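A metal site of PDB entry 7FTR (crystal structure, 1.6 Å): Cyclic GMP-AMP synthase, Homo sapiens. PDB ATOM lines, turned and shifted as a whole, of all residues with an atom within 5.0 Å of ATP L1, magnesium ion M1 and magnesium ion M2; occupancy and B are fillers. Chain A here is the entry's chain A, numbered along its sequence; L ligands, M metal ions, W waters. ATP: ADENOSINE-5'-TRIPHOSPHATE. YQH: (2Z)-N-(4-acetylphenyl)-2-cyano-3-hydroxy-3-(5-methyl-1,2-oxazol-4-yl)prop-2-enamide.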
ATOM      1  N   GLY A  52       5.928  24.982  21.087  1.00  0.00           N
ATOM      2  CA  GLY A  52       6.414  24.485  22.367  1.00  0.00           C
ATOM      3  C   GLY A  52       5.834  25.196  23.559  1.00  0.00           C
ATOM      4  O   GLY A  52       4.910  26.014  23.434  1.00  0.00           O
ATOM      5  N   SER A  53       6.331  24.835  24.748  1.00  0.00           N
ATOM      6  CA  SER A  53       5.689  25.239  26.002  1.00  0.00           C
ATOM      7  C   SER A  53       5.684  26.727  26.248  1.00  0.00           C
ATOM      8  O   SER A  53       4.707  27.230  26.818  1.00  0.00           O
ATOM      9  CB  SER A  53       6.283  24.500  27.188  1.00  0.00           C
ATOM     10  OG  SER A  53       7.652  24.832  27.269  1.00  0.00           O
ATOM     11  N   GLU A  56       2.797  28.116  24.353  1.00  0.00           N
ATOM     12  CA  GLU A  56       1.562  27.501  24.863  1.00  0.00           C
ATOM     13  C   GLU A  56       1.292  27.977  26.298  1.00  0.00           C
ATOM     14  O   GLU A  56       0.282  27.591  26.891  1.00  0.00           O
ATOM     15  CB  GLU A  56       1.761  25.991  24.915  1.00  0.00           C
ATOM     16  CG  GLU A  56       1.791  25.375  23.533  1.00  0.00           C
ATOM     17  CD  GLU A  56       2.372  23.983  23.471  1.00  0.00           C
ATOM     18  OE1 GLU A  56       3.010  23.558  24.453  1.00  0.00           O
ATOM     19  OE2 GLU A  56       2.195  23.325  22.420  1.00  0.00           O
ATOM     20  N   LYS A  59       5.271  26.634  29.965  1.00  0.00           N
ATOM     21  CA  LYS A  59       6.693  26.593  30.344  1.00  0.00           C
ATOM     22  C   LYS A  59       6.720  26.863  31.840  1.00  0.00           C
ATOM     23  O   LYS A  59       5.994  27.734  32.327  1.00  0.00           O
ATOM     24  CB  LYS A  59       7.474  27.697  29.615  1.00  0.00           C
ATOM     25  CG  LYS A  59       8.963  27.744  29.952  1.00  0.00           C
ATOM     26  CD  LYS A  59       9.730  26.616  29.289  1.00  0.00           C
ATOM     27  CE  LYS A  59      11.183  26.481  29.711  1.00  0.00           C
ATOM     28  NZ  LYS A  59      11.342  26.155  31.169  1.00  0.00           N
ATOM     29  N   GLU A  65      13.874  28.113  27.591  1.00  0.00           N
ATOM     30  CA  GLU A  65      13.902  27.173  26.473  1.00  0.00           C
ATOM     31  C   GLU A  65      12.717  27.473  25.573  1.00  0.00           C
ATOM     32  O   GLU A  65      11.562  27.432  26.007  1.00  0.00           O
ATOM     33  CB  GLU A  65      13.974  25.699  26.928  1.00  0.00           C
ATOM     34  CG  GLU A  65      14.444  24.736  25.842  1.00  0.00           C
ATOM     35  CD  GLU A  65      13.343  24.000  25.095  1.00  0.00           C
ATOM     36  OE1 GLU A  65      12.156  24.269  25.337  1.00  0.00           O
ATOM     37  OE2 GLU A  65      13.678  23.139  24.254  1.00  0.00           O
ATOM     38  N   ASP A  67      11.143  27.049  21.565  1.00  0.00           N
ATOM     39  CA  ASP A  67      11.111  26.167  20.413  1.00  0.00           C
ATOM     40  C   ASP A  67      10.527  26.935  19.265  1.00  0.00           C
ATOM     41  O   ASP A  67       9.543  27.681  19.410  1.00  0.00           O
ATOM     42  CB  ASP A  67      10.311  24.909  20.725  1.00  0.00           C
ATOM     43  CG  ASP A  67      10.863  24.184  21.937  1.00  0.00           C
ATOM     44  OD1 ASP A  67      11.896  23.485  21.786  1.00  0.00           O
ATOM     45  OD2 ASP A  67      10.219  24.288  23.049  1.00  0.00           O
ATOM     46  N   ASP A 159      15.644  25.946  20.494  1.00  0.00           N
ATOM     47  CA  ASP A 159      15.630  24.785  19.619  1.00  0.00           C
ATOM     48  C   ASP A 159      14.979  25.188  18.332  1.00  0.00           C
ATOM     49  O   ASP A 159      13.809  25.609  18.322  1.00  0.00           O
ATOM     50  CB  ASP A 159      14.873  23.587  20.241  1.00  0.00           C
ATOM     51  CG  ASP A 159      15.562  22.870  21.360  1.00  0.00           C
ATOM     52  OD1 ASP A 159      16.797  23.027  21.504  1.00  0.00           O
ATOM     53  OD2 ASP A 159      14.888  22.110  22.066  1.00  0.00           O
ATOM     54  N   ARG A 216       9.851  12.917  10.225  1.00  0.00           N
ATOM     55  CA  ARG A 216       8.715  12.560  11.085  1.00  0.00           C
ATOM     56  C   ARG A 216       7.649  13.638  11.085  1.00  0.00           C
ATOM     57  O   ARG A 216       7.980  14.830  11.017  1.00  0.00           O
ATOM     58  CB  ARG A 216       9.158  12.275  12.539  1.00  0.00           C
ATOM     59  CG  ARG A 216       8.080  11.495  13.336  1.00  0.00           C
ATOM     60  CD  ARG A 216       8.094  11.769  14.812  1.00  0.00           C
ATOM     61  NE  ARG A 216       7.678  13.161  15.016  1.00  0.00           N
ATOM     62  CZ  ARG A 216       8.378  14.072  15.677  1.00  0.00           C
ATOM     63  NH1 ARG A 216       7.965  15.334  15.702  1.00  0.00           N
ATOM     64  NH2 ARG A 216       9.479  13.729  16.343  1.00  0.00           N
ATOM     65  N   LEU A 217       6.367  13.215  11.205  1.00  0.00           N
ATOM     66  CA  LEU A 217       5.245  14.145  11.275  1.00  0.00           C
ATOM     67  C   LEU A 217       5.326  14.989  12.533  1.00  0.00           C
ATOM     68  O   LEU A 217       5.680  14.495  13.608  1.00  0.00           O
ATOM     69  CB  LEU A 217       3.864  13.449  11.198  1.00  0.00           C
ATOM     70  CG  LEU A 217       3.492  12.746   9.879  1.00  0.00           C
ATOM     71  CD1 LEU A 217       2.134  12.049   9.986  1.00  0.00           C
ATOM     72  CD2 LEU A 217       3.444  13.727   8.726  1.00  0.00           C
ATOM     73  N   SER A 220       3.091  20.355  16.049  1.00  0.00           N
ATOM     74  CA  SER A 220       3.386  21.374  17.088  1.00  0.00           C
ATOM     75  C   SER A 220       2.462  22.597  16.999  1.00  0.00           C
ATOM     76  O   SER A 220       2.080  23.164  18.035  1.00  0.00           O
ATOM     77  CB  SER A 220       4.831  21.844  16.939  1.00  0.00           C
ATOM     78  OG  SER A 220       5.730  20.770  17.114  1.00  0.00           O
ATOM     79  N   GLU A 223      -0.895  21.557  18.394  1.00  0.00           N
ATOM     80  CA  GLU A 223      -0.798  21.424  19.851  1.00  0.00           C
ATOM     81  C   GLU A 223      -0.860  22.803  20.494  1.00  0.00           C
ATOM     82  O   GLU A 223      -1.525  22.970  21.500  1.00  0.00           O
ATOM     83  CB  GLU A 223       0.516  20.725  20.242  1.00  0.00           C
ATOM     84  CG  GLU A 223       0.568  19.292  19.737  1.00  0.00           C
ATOM     85  CD  GLU A 223       1.933  18.624  19.793  1.00  0.00           C
ATOM     86  OE1 GLU A 223       2.814  19.169  20.495  1.00  0.00           O
ATOM     87  OE2 GLU A 223       2.121  17.567  19.170  1.00  0.00           O
ATOM     88  N   LYS A 254       4.503  18.161  34.251  1.00  0.00           N
ATOM     89  CA  LYS A 254       5.849  18.451  33.736  1.00  0.00           C
ATOM     90  C   LYS A 254       6.840  18.547  34.874  1.00  0.00           C
ATOM     91  O   LYS A 254       7.956  18.047  34.744  1.00  0.00           O
ATOM     92  CB  LYS A 254       5.854  19.790  32.955  1.00  0.00           C
ATOM     93  CG  LYS A 254       5.007  19.737  31.689  1.00  0.00           C
ATOM     94  CD  LYS A 254       4.809  21.115  31.020  1.00  0.00           C
ATOM     95  CE  LYS A 254       6.107  21.851  30.715  1.00  0.00           C
ATOM     96  NZ  LYS A 254       6.928  21.070  29.741  1.00  0.00           N
ATOM     97  N   GLU A 258      10.210  16.412  35.640  1.00  0.00           N
ATOM     98  CA  GLU A 258      11.486  17.122  35.701  1.00  0.00           C
ATOM     99  C   GLU A 258      12.187  16.838  37.053  1.00  0.00           C
ATOM    100  O   GLU A 258      13.415  16.604  37.088  1.00  0.00           O
ATOM    101  CB  GLU A 258      11.289  18.650  35.546  1.00  0.00           C
ATOM    102  CG  GLU A 258      10.962  19.165  34.154  1.00  0.00           C
ATOM    103  CD  GLU A 258      11.027  20.678  33.991  1.00  0.00           C
ATOM    104  OE1 GLU A 258      11.593  21.344  34.890  1.00  0.00           O
ATOM    105  OE2 GLU A 258      10.519  21.199  32.970  1.00  0.00           O
ATOM    106  N   SER A 275       9.261  15.597  28.406  1.00  0.00           N
ATOM    107  CA  SER A 275       8.039  16.366  28.698  1.00  0.00           C
ATOM    108  C   SER A 275       6.978  16.060  27.654  1.00  0.00           C
ATOM    109  O   SER A 275       5.803  16.180  27.949  1.00  0.00           O
ATOM    110  CB  SER A 275       8.348  17.865  28.710  1.00  0.00           C
ATOM    111  OG  SER A 275       8.812  18.255  27.433  1.00  0.00           O
ATOM    112  N   TYR A 276       7.381  15.705  26.408  1.00  0.00           N
ATOM    113  CA  TYR A 276       6.392  15.335  25.368  1.00  0.00           C
ATOM    114  C   TYR A 276       5.523  14.113  25.743  1.00  0.00           C
ATOM    115  O   TYR A 276       4.355  14.033  25.334  1.00  0.00           O
ATOM    116  CB  TYR A 276       7.023  15.110  23.985  1.00  0.00           C
ATOM    117  CG  TYR A 276       5.989  15.128  22.875  1.00  0.00           C
ATOM    118  CD1 TYR A 276       5.244  16.285  22.602  1.00  0.00           C
ATOM    119  CD2 TYR A 276       5.684  13.975  22.157  1.00  0.00           C
ATOM    120  CE1 TYR A 276       4.236  16.279  21.635  1.00  0.00           C
ATOM    121  CE2 TYR A 276       4.676  13.968  21.190  1.00  0.00           C
ATOM    122  CZ  TYR A 276       4.005  15.139  20.882  1.00  0.00           C
ATOM    123  OH  TYR A 276       3.025  15.114  19.928  1.00  0.00           O
ATOM    124  N   LYS A 279       2.951  15.671  27.986  1.00  0.00           N
ATOM    125  CA  LYS A 279       2.057  16.504  27.192  1.00  0.00           C
ATOM    126  C   LYS A 279       1.066  15.621  26.440  1.00  0.00           C
ATOM    127  O   LYS A 279      -0.136  15.915  26.436  1.00  0.00           O
ATOM    128  CB  LYS A 279       2.886  17.339  26.216  1.00  0.00           C
ATOM    129  CG  LYS A 279       2.054  18.445  25.559  1.00  0.00           C
ATOM    130  CD  LYS A 279       2.918  19.066  24.439  1.00  0.00           C
ATOM    131  CE  LYS A 279       2.268  20.314  23.910  1.00  0.00           C
ATOM    132  NZ  LYS A 279       3.055  20.817  22.759  1.00  0.00           N
ATOM    133  N   ASN A 322       0.660   8.555  20.169  1.00  0.00           N
ATOM    134  CA  ASN A 322       0.888   9.935  19.747  1.00  0.00           C
ATOM    135  C   ASN A 322      -0.572  10.445  19.516  1.00  0.00           C
ATOM    136  O   ASN A 322      -1.414   9.727  18.974  1.00  0.00           O
ATOM    137  CB  ASN A 322       1.703   9.941  18.445  1.00  0.00           C
ATOM    138  CG  ASN A 322       1.781  11.288  17.760  1.00  0.00           C
ATOM    139  OD1 ASN A 322       0.795  11.832  17.268  1.00  0.00           O
ATOM    140  ND2 ASN A 322       2.979  11.840  17.695  1.00  0.00           N
ATOM    141  N   LEU A 330       4.462   5.788  21.635  1.00  0.00           N
ATOM    142  CA  LEU A 330       5.618   6.422  22.256  1.00  0.00           C
ATOM    143  C   LEU A 330       6.233   5.545  23.370  1.00  0.00           C
ATOM    144  O   LEU A 330       7.417   5.718  23.693  1.00  0.00           O
ATOM    145  CB  LEU A 330       5.228   7.803  22.861  1.00  0.00           C
ATOM    146  CG  LEU A 330       4.531   8.838  21.919  1.00  0.00           C
ATOM    147  CD1 LEU A 330       4.218  10.086  22.658  1.00  0.00           C
ATOM    148  CD2 LEU A 330       5.424   9.217  20.789  1.00  0.00           C
HETATM  149  PG  ATP L   1       9.455  21.947  27.632  1.00  0.00           P
HETATM  150  O1G ATP L   1      10.394  22.649  26.678  1.00  0.00           O
HETATM  151  O2G ATP L   1       9.930  20.685  28.289  1.00  0.00           O
HETATM  152  O3G ATP L   1       8.873  22.819  28.696  1.00  0.00           O
HETATM  153  PB  ATP L   1       8.009  21.543  25.166  1.00  0.00           P
HETATM  154  O1B ATP L   1       6.613  21.192  24.760  1.00  0.00           O
HETATM  155  O2B ATP L   1       8.429  22.863  24.521  1.00  0.00           O
HETATM  156  O3B ATP L   1       8.196  21.584  26.739  1.00  0.00           O
HETATM  157  PA  ATP L   1      10.202  20.300  23.616  1.00  0.00           P
HETATM  158  O1A ATP L   1      11.020  19.130  24.017  1.00  0.00           O
HETATM  159  O2A ATP L   1      10.909  21.618  23.844  1.00  0.00           O
HETATM  160  O3A ATP L   1       8.984  20.392  24.641  1.00  0.00           O
HETATM  161  O5' ATP L   1       9.598  20.248  22.177  1.00  0.00           O
HETATM  162  C5' ATP L   1       8.953  21.336  21.524  1.00  0.00           C
HETATM  163  C4' ATP L   1       7.793  20.760  20.758  1.00  0.00           C
HETATM  164  O4' ATP L   1       8.285  19.761  19.846  1.00  0.00           O
HETATM  165  C3' ATP L   1       6.754  20.013  21.588  1.00  0.00           C
HETATM  166  O3' ATP L   1       5.838  20.908  22.216  1.00  0.00           O
HETATM  167  C2' ATP L   1       6.088  19.143  20.535  1.00  0.00           C
HETATM  168  O2' ATP L   1       5.186  19.916  19.757  1.00  0.00           O
HETATM  169  C1' ATP L   1       7.299  18.764  19.648  1.00  0.00           C
HETATM  170  N9  ATP L   1       7.881  17.471  19.976  1.00  0.00           N
HETATM  171  C8  ATP L   1       8.854  17.190  20.906  1.00  0.00           C
HETATM  172  N7  ATP L   1       9.098  15.909  21.059  1.00  0.00           N
HETATM  173  C5  ATP L   1       8.245  15.300  20.152  1.00  0.00           C
HETATM  174  C6  ATP L   1       8.036  13.957  19.796  1.00  0.00           C
HETATM  175  N6  ATP L   1       8.682  12.933  20.370  1.00  0.00           N
HETATM  176  N1  ATP L   1       7.092  13.693  18.874  1.00  0.00           N
HETATM  177  C2  ATP L   1       6.405  14.699  18.330  1.00  0.00           C
HETATM  178  N3  ATP L   1       6.529  16.016  18.565  1.00  0.00           N
HETATM  179  C4  ATP L   1       7.480  16.249  19.483  1.00  0.00           C
HETATM  180  C10 YQH L   2      10.599  17.201  17.853  1.00  0.00           C
HETATM  181  C11 YQH L   2       9.081  18.646  16.548  1.00  0.00           C
HETATM  182  C15 YQH L   2      12.251  15.918  19.261  1.00  0.00           C
HETATM  183  C16 YQH L   2      11.692  14.640  19.223  1.00  0.00           C
HETATM  184  C17 YQH L   2      13.509  16.086  19.847  1.00  0.00           C
HETATM  185  C18 YQH L   2      12.389  13.548  19.726  1.00  0.00           C
HETATM  186  C19 YQH L   2      14.200  14.992  20.358  1.00  0.00           C
HETATM  187  C20 YQH L   2      13.654  13.707  20.290  1.00  0.00           C
HETATM  188  C21 YQH L   2      14.389  12.525  20.841  1.00  0.00           C
HETATM  189  C22 YQH L   2      15.752  12.713  21.438  1.00  0.00           C
HETATM  190  C1  YQH L   2      10.214  21.108  17.665  1.00  0.00           C
HETATM  191  C2  YQH L   2      10.675  19.742  17.970  1.00  0.00           C
HETATM  192  C3  YQH L   2      10.839  22.314  17.811  1.00  0.00           C
HETATM  193  C4  YQH L   2       8.930  21.448  17.185  1.00  0.00           C
HETATM  194  C5  YQH L   2      10.149  18.559  17.504  1.00  0.00           C
HETATM  195  O6  YQH L   2      11.645  19.715  18.867  1.00  0.00           O
HETATM  196  O7  YQH L   2      10.001  23.296  17.443  1.00  0.00           O
HETATM  197  C8  YQH L   2      12.178  22.739  18.273  1.00  0.00           C
HETATM  198  N9  YQH L   2       8.776  22.729  17.039  1.00  0.00           N
HETATM  199  N12 YQH L   2      11.603  17.080  18.772  1.00  0.00           N
HETATM  200  O13 YQH L   2      10.044  16.225  17.351  1.00  0.00           O
HETATM  201  N14 YQH L   2       8.265  18.667  15.758  1.00  0.00           N
HETATM  202  O23 YQH L   2      13.890  11.399  20.797  1.00  0.00           O
HETATM  203 MG    MG M   1      12.879  21.901  22.776  1.00  0.00          MG
HETATM  204 MG    MG M   2      10.366  23.479  24.807  1.00  0.00          MG
HETATM  205  O   HOH W   1       9.190  23.749  31.060  1.00  0.00           O
HETATM  206  O   HOH W   2      10.020  16.826  25.101  1.00  0.00           O
HETATM  207  O   HOH W   3      12.930  17.761  22.776  1.00  0.00           O
HETATM  208  O   HOH W   4      10.180  12.260  23.165  1.00  0.00           O
HETATM  209  O   HOH W   5       9.799  25.313  25.711  1.00  0.00           O
HETATM  210  O   HOH W   6      12.021  18.906  26.447  1.00  0.00           O
HETATM  211  O   HOH W   7       3.794  16.942  17.079  1.00  0.00           O
HETATM  212  O   HOH W   8       6.405  18.623  25.825  1.00  0.00           O
HETATM  213  O   HOH W   9       5.629  11.425  18.207  1.00  0.00           O
HETATM  214  O   HOH W  10       8.916  19.874  31.313  1.00  0.00           O
HETATM  215  O   HOH W  11       8.991   9.556  20.942  1.00  0.00           O
HETATM  216  O   HOH W  12      12.655  20.692  21.052  1.00  0.00           O
HETATM  217  O   HOH W  13       4.230  21.805  26.143  1.00  0.00           O
HETATM  218  O   HOH W  14      11.887  20.202  30.503  1.00  0.00           O
HETATM  219  O   HOH W  15      13.645  20.553  23.934  1.00  0.00           O
HETATM  220  O   HOH W  16      10.971  15.422  22.940  1.00  0.00           O
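A nitrogen (N3) of ATP L1 sits close to the guanidinium group of Arg 216 (3.3 Å).
An oxygen (O2') of ATP L1 lies within hydrogen-bond range of the side-chain hydroxyl (OG) of Ser 220.
The side-chain hydroxyl of Ser 275 sits at hydrogen-bond distance from an oxygen (O2G) of ATP L1 (2.8 Å).
The side-chain carboxylate (OE1) of Glu 223 is in hydrogen-bond range of an oxygen (O2') of ATP L1 (2.6 Å).
An oxygen (O3G) of ATP L1 is in hydrogen-bond range of the side-chain hydroxyl of Ser 53, at 2.8 Å.
NH2 of Arg 216 lies within hydrogen-bond range of O13 of YQH L2 (2.8 Å).
The side-chain amino group (NZ) of Lys 254 lies within salt-bridge range of an oxygen (O3G) of ATP L1 (2.8 Å).
NZ of Lys 279 lies within hydrogen-bond range of O3' of ATP L1 (2.8 Å).
The backbone NH of Ser 53 lies close to an oxygen (O2B) of ATP L1 (2.9 Å).
O4' of ATP L1 lies close to O6 of YQH L2, 3.5 Å away.
N of Lys 59 is in hydrogen-bond range of O of Ser 53 (3.3 Å).
The side-chain carboxylate (OE2) of Glu 56 lies within salt-bridge range of the side-chain amino group (NZ) of Lys 279.
OH of Tyr 276 sits at hydrogen-bond distance from OE2 of Glu 223 (2.7 Å).
The side-chain carboxylate of Glu 223 is in salt-bridge range of the side-chain amino group of Lys 279, 2.8 Å away.
Gly 52 touches ATP L1 (CA to O2B, 3.4 Å).
CD of Lys 59 touches O3G of ATP L1 (3.9 Å).
Tyr 276 touches ATP L1 (CD2 to C6, 3.3 Å).
Of the 18 residues printed, 12 come within 4 Å of ATP L1.
Along chain A the residues within 4 Å of ATP L1 span positions 52 to 279.
The nearest printed residue that does not touch ATP L1 is Glu 56 (4.3 Å).
Of the 18 residues printed, 3 come within 4 Å of magnesium ion M1.
The nearest printed residue that does not touch magnesium ion M1 is Gly 52 (7.0 Å).
Residues that only touch magnesium ion M2: Ser 53.
Magnesium ion M1 is bound by water W15, OE2 of Glu 65, OD1 of Asp 67, water W12, OD2 of Asp 159 and O2A of ATP L1.
Magnesium ion M2 is bound by the side-chain carboxylate (OD2) of Asp 67 (1.9 Å), the side-chain carboxylate (OE1) of Glu 65 (2.0 Å), an oxygen (O1G) of ATP L1 (2.0 Å), an oxygen (O2B) of ATP L1 (2.1 Å), water W5 (2.1 Å) and an oxygen (O2A) of ATP L1 (2.2 Å).
Water W5 bridges the side-chain hydroxyl of Ser 53 (2.7 Å) and the backbone carbonyl oxygen of Glu 65 (2.8 Å).
Water W6 bridges O1A of ATP L1 and OG of Ser 275.
Water W2 lies within hydrogen-bond range of O1A of ATP L1 (2.7 Å), OG of Ser 275 (3.0 Å) and N of Tyr 276 (3.2 Å).
Water W9 bridges ND2 of Asn 322 (2.7 Å) and N1 of ATP L1 (2.8 Å).
Water W13 lies within hydrogen-bond range of OE1 of Glu 56 (2.7 Å) and O1B of ATP L1 (2.8 Å).
Water W7 lies within hydrogen-bond range of the side-chain carboxylate (OE2) of Glu 223 (2.7 Å), a nitrogen (N3) of ATP L1 (3.2 Å) and the side-chain hydroxyl (OH) of Tyr 276 (3.5 Å).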
